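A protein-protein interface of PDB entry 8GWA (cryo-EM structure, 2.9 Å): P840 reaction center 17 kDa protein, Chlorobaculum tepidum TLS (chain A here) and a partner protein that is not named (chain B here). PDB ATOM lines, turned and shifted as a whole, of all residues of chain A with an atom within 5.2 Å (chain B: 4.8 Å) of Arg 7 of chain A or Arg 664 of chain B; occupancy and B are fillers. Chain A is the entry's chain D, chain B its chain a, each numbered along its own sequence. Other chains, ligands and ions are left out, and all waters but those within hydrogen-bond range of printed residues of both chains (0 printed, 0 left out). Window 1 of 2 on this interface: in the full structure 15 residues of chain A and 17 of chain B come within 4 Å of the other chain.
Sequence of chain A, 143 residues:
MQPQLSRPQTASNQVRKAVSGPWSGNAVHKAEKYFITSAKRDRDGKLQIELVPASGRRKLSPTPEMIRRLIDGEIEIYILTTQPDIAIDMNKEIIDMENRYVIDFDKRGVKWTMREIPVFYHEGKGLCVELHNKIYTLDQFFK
The side-chain amide oxygen (OE1) of Gln 9 of chain A sits close to the side-chain amide oxygen (OD1) of Asn 662 of chain B (3.1 Å). OE1 of Gln 9 of chain A lies close to NH2 of Arg 664 of chain B. The guanidinium group (NH1) of Arg 647 of chain B sits at hydrogen-bond distance from the backbone carbonyl oxygen (O) of Leu 5 of chain A (3.1 Å). NE of Arg 7 of chain A is in salt-bridge range of OD1 of Asp 643 of chain B, at 3.1 Å.
OG1 of Thr 646 of chain B is in hydrogen-bond range of N of Phe 665 of chain B. NE of Arg 647 of chain B is in salt-bridge range of OD1 of Asp 643 of chain B (2.8 Å).
Among the printed residues, pairs that only touch across the chains: Ser 6 of chain A with Arg 647 of chain B, Arg 7 of chain A with Thr 646 of chain B, Arg 7 of chain A with Arg 647 of chain B, Arg 7 of chain A with Arg 664 of chain B, Pro 8 of chain A with Thr 646 of chain B and Pro 8 of chain A with Asn 662 of chain B.
Printed residues of chain B within 4 Å of Leu 5 of chain A: Arg 647. Of the printed residues of chain B, Ser 6 of chain A touches Arg 647 (3.3 Å). Phe 663 of chain B touches none of the printed residues of chain A. Arg 664 of chain B touches just these residues of chain A: Arg 7 (3.4 Å) and Gln 9 (2.3 Å). Phe 665 of chain B touches none of the printed residues of chain A.
Of the 9 printed residues of chain B, 5 touch a printed residue of chain A. Printed residues of chain A that touch a printed residue of chain B: Leu 5, Ser 6, Arg 7, Pro 8 and Gln 9.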
ATOM      1  N   LEU A   5       3.641  24.161  29.184  1.00  0.00           N
ATOM      2  CA  LEU A   5       3.353  25.545  29.526  1.00  0.00           C
ATOM      3  C   LEU A   5       3.898  26.517  28.490  1.00  0.00           C
ATOM      4  O   LEU A   5       3.867  27.731  28.715  1.00  0.00           O
ATOM      5  CB  LEU A   5       3.923  25.876  30.907  1.00  0.00           C
ATOM      6  CG  LEU A   5       3.007  25.590  32.098  1.00  0.00           C
ATOM      7  CD1 LEU A   5       3.777  25.712  33.398  1.00  0.00           C
ATOM      8  CD2 LEU A   5       1.810  26.521  32.093  1.00  0.00           C
ATOM      9  N   SER A   6       4.386  26.015  27.362  1.00  0.00           N
ATOM     10  CA  SER A   6       4.995  26.837  26.331  1.00  0.00           C
ATOM     11  C   SER A   6       4.170  26.770  25.053  1.00  0.00           C
ATOM     12  O   SER A   6       3.291  25.917  24.898  1.00  0.00           O
ATOM     13  CB  SER A   6       6.437  26.395  26.047  1.00  0.00           C
ATOM     14  OG  SER A   6       6.493  25.011  25.748  1.00  0.00           O
ATOM     15  N   ARG A   7       4.459  27.694  24.144  1.00  0.00           N
ATOM     16  CA  ARG A   7       3.800  27.695  22.850  1.00  0.00           C
ATOM     17  C   ARG A   7       4.112  26.384  22.127  1.00  0.00           C
ATOM     18  O   ARG A   7       5.250  25.905  22.184  1.00  0.00           O
ATOM     19  CB  ARG A   7       4.263  28.900  22.029  1.00  0.00           C
ATOM     20  CG  ARG A   7       3.428  29.210  20.800  1.00  0.00           C
ATOM     21  CD  ARG A   7       2.105  29.846  21.197  1.00  0.00           C
ATOM     22  NE  ARG A   7       2.215  31.284  21.408  1.00  0.00           N
ATOM     23  CZ  ARG A   7       1.969  32.198  20.479  1.00  0.00           C
ATOM     24  NH1 ARG A   7       1.596  31.858  19.257  1.00  0.00           N
ATOM     25  NH2 ARG A   7       2.098  33.485  20.786  1.00  0.00           N
ATOM     26  N   PRO A   8       3.120  25.769  21.456  1.00  0.00           N
ATOM     27  CA  PRO A   8       3.257  24.372  21.012  1.00  0.00           C
ATOM     28  C   PRO A   8       4.547  24.011  20.289  1.00  0.00           C
ATOM     29  O   PRO A   8       5.265  23.109  20.733  1.00  0.00           O
ATOM     30  CB  PRO A   8       2.051  24.198  20.083  1.00  0.00           C
ATOM     31  CG  PRO A   8       1.023  25.115  20.642  1.00  0.00           C
ATOM     32  CD  PRO A   8       1.732  26.249  21.334  1.00  0.00           C
ATOM     33  N   GLN A   9       4.864  24.689  19.188  1.00  0.00           N
ATOM     34  CA  GLN A   9       6.054  24.352  18.408  1.00  0.00           C
ATOM     35  C   GLN A   9       7.235  25.172  18.916  1.00  0.00           C
ATOM     36  O   GLN A   9       7.670  26.153  18.308  1.00  0.00           O
ATOM     37  CB  GLN A   9       5.810  24.571  16.921  1.00  0.00           C
ATOM     38  CG  GLN A   9       5.115  23.412  16.229  1.00  0.00           C
ATOM     39  CD  GLN A   9       3.612  23.524  16.263  1.00  0.00           C
ATOM     40  OE1 GLN A   9       3.063  24.569  16.607  1.00  0.00           O
ATOM     41  NE2 GLN A   9       2.932  22.444  15.897  1.00  0.00           N
ATOM     42  N   THR A  10       7.764  24.749  20.063  1.00  0.00           N
ATOM     43  CA  THR A  10       8.952  25.347  20.657  1.00  0.00           C
ATOM     44  C   THR A  10      10.024  24.274  20.771  1.00  0.00           C
ATOM     45  O   THR A  10       9.798  23.232  21.396  1.00  0.00           O
ATOM     46  CB  THR A  10       8.649  25.947  22.031  1.00  0.00           C
ATOM     47  OG1 THR A  10       7.414  26.670  21.974  1.00  0.00           O
ATOM     48  CG2 THR A  10       9.753  26.904  22.443  1.00  0.00           C
ATOM     49  N   LEU B 639      -2.422  40.022  22.258  1.00  0.00           N
ATOM     50  CA  LEU B 639      -1.516  38.970  21.811  1.00  0.00           C
ATOM     51  C   LEU B 639      -0.829  38.287  22.989  1.00  0.00           C
ATOM     52  O   LEU B 639      -0.730  37.053  23.032  1.00  0.00           O
ATOM     53  CB  LEU B 639      -0.485  39.555  20.849  1.00  0.00           C
ATOM     54  CG  LEU B 639       0.719  38.680  20.517  1.00  0.00           C
ATOM     55  CD1 LEU B 639       0.272  37.412  19.810  1.00  0.00           C
ATOM     56  CD2 LEU B 639       1.721  39.460  19.683  1.00  0.00           C
ATOM     57  N   ASP B 643      -1.385  34.390  24.064  1.00  0.00           N
ATOM     58  CA  ASP B 643      -0.338  33.409  24.322  1.00  0.00           C
ATOM     59  C   ASP B 643      -0.528  32.793  25.701  1.00  0.00           C
ATOM     60  O   ASP B 643      -0.316  31.587  25.890  1.00  0.00           O
ATOM     61  CB  ASP B 643       1.043  34.051  24.189  1.00  0.00           C
ATOM     62  CG  ASP B 643       2.171  33.028  24.236  1.00  0.00           C
ATOM     63  OD1 ASP B 643       1.897  31.822  24.400  1.00  0.00           O
ATOM     64  OD2 ASP B 643       3.343  33.425  24.089  1.00  0.00           O
ATOM     65  N   THR B 646      -3.181  30.230  25.234  1.00  0.00           N
ATOM     66  CA  THR B 646      -2.638  29.036  24.596  1.00  0.00           C
ATOM     67  C   THR B 646      -1.901  28.168  25.607  1.00  0.00           C
ATOM     68  O   THR B 646      -2.117  26.951  25.675  1.00  0.00           O
ATOM     69  CB  THR B 646      -1.706  29.434  23.451  1.00  0.00           C
ATOM     70  OG1 THR B 646      -2.435  30.191  22.478  1.00  0.00           O
ATOM     71  CG2 THR B 646      -1.112  28.200  22.794  1.00  0.00           C
ATOM     72  N   ARG B 647      -1.032  28.785  26.411  1.00  0.00           N
ATOM     73  CA  ARG B 647      -0.275  28.022  27.398  1.00  0.00           C
ATOM     74  C   ARG B 647      -1.189  27.430  28.462  1.00  0.00           C
ATOM     75  O   ARG B 647      -0.925  26.338  28.974  1.00  0.00           O
ATOM     76  CB  ARG B 647       0.797  28.901  28.037  1.00  0.00           C
ATOM     77  CG  ARG B 647       1.758  29.512  27.041  1.00  0.00           C
ATOM     78  CD  ARG B 647       2.529  30.661  27.651  1.00  0.00           C
ATOM     79  NE  ARG B 647       3.409  31.288  26.674  1.00  0.00           N
ATOM     80  CZ  ARG B 647       4.684  30.966  26.502  1.00  0.00           C
ATOM     81  NH1 ARG B 647       5.264  30.028  27.232  1.00  0.00           N
ATOM     82  NH2 ARG B 647       5.394  31.607  25.580  1.00  0.00           N
ATOM     83  N   ASN B 662      -1.905  21.449  20.418  1.00  0.00           N
ATOM     84  CA  ASN B 662      -1.191  22.271  19.441  1.00  0.00           C
ATOM     85  C   ASN B 662      -1.912  23.553  19.029  1.00  0.00           C
ATOM     86  O   ASN B 662      -1.261  24.517  18.613  1.00  0.00           O
ATOM     87  CB  ASN B 662      -0.898  21.424  18.199  1.00  0.00           C
ATOM     88  CG  ASN B 662      -0.215  22.211  17.101  1.00  0.00           C
ATOM     89  OD1 ASN B 662       1.004  22.354  17.097  1.00  0.00           O
ATOM     90  ND2 ASN B 662      -0.999  22.717  16.156  1.00  0.00           N
ATOM     91  N   PHE B 663      -3.242  23.573  19.101  1.00  0.00           N
ATOM     92  CA  PHE B 663      -3.986  24.789  18.794  1.00  0.00           C
ATOM     93  C   PHE B 663      -3.489  25.971  19.621  1.00  0.00           C
ATOM     94  O   PHE B 663      -3.237  25.850  20.823  1.00  0.00           O
ATOM     95  CB  PHE B 663      -5.480  24.581  19.048  1.00  0.00           C
ATOM     96  CG  PHE B 663      -6.281  25.854  19.024  1.00  0.00           C
ATOM     97  CD1 PHE B 663      -6.707  26.402  17.826  1.00  0.00           C
ATOM     98  CD2 PHE B 663      -6.610  26.503  20.205  1.00  0.00           C
ATOM     99  CE1 PHE B 663      -7.440  27.574  17.808  1.00  0.00           C
ATOM    100  CE2 PHE B 663      -7.340  27.675  20.190  1.00  0.00           C
ATOM    101  CZ  PHE B 663      -7.755  28.211  18.991  1.00  0.00           C
ATOM    102  N   ARG B 664      -3.350  27.120  18.962  1.00  0.00           N
ATOM    103  CA  ARG B 664      -2.990  28.368  19.618  1.00  0.00           C
ATOM    104  C   ARG B 664      -4.011  29.439  19.260  1.00  0.00           C
ATOM    105  O   ARG B 664      -4.552  29.460  18.152  1.00  0.00           O
ATOM    106  CB  ARG B 664      -1.575  28.829  19.230  1.00  0.00           C
ATOM    107  CG  ARG B 664      -1.429  29.320  17.800  1.00  0.00           C
ATOM    108  CD  ARG B 664       0.035  29.429  17.405  1.00  0.00           C
ATOM    109  NE  ARG B 664       0.579  28.157  16.948  1.00  0.00           N
ATOM    110  CZ  ARG B 664       1.869  27.918  16.760  1.00  0.00           C
ATOM    111  NH1 ARG B 664       2.784  28.847  16.990  1.00  0.00           N
ATOM    112  NH2 ARG B 664       2.252  26.719  16.333  1.00  0.00           N
ATOM    113  N   PHE B 665      -4.274  30.325  20.214  1.00  0.00           N
ATOM    114  CA  PHE B 665      -5.301  31.343  20.033  1.00  0.00           C
ATOM    115  C   PHE B 665      -4.810  32.431  19.084  1.00  0.00           C
ATOM    116  O   PHE B 665      -3.736  32.998  19.304  1.00  0.00           O
ATOM    117  CB  PHE B 665      -5.690  31.960  21.371  1.00  0.00           C
ATOM    118  CG  PHE B 665      -6.569  31.080  22.208  1.00  0.00           C
ATOM    119  CD1 PHE B 665      -6.026  30.062  22.970  1.00  0.00           C
ATOM    120  CD2 PHE B 665      -7.938  31.268  22.229  1.00  0.00           C
ATOM    121  CE1 PHE B 665      -6.832  29.249  23.738  1.00  0.00           C
ATOM    122  CE2 PHE B 665      -8.750  30.457  22.997  1.00  0.00           C
ATOM    123  CZ  PHE B 665      -8.196  29.447  23.752  1.00  0.00           C
ATOM    124  N   PRO B 666      -5.561  32.747  18.033  1.00  0.00           N
ATOM    125  CA  PRO B 666      -5.165  33.823  17.124  1.00  0.00           C
ATOM    126  C   PRO B 666      -5.696  35.179  17.558  1.00  0.00           C
ATOM    127  O   PRO B 666      -6.781  35.308  18.128  1.00  0.00           O
ATOM    128  CB  PRO B 666      -5.797  33.390  15.794  1.00  0.00           C
ATOM    129  CG  PRO B 666      -7.021  32.633  16.202  1.00  0.00           C
ATOM    130  CD  PRO B 666      -6.773  32.047  17.572  1.00  0.00           C
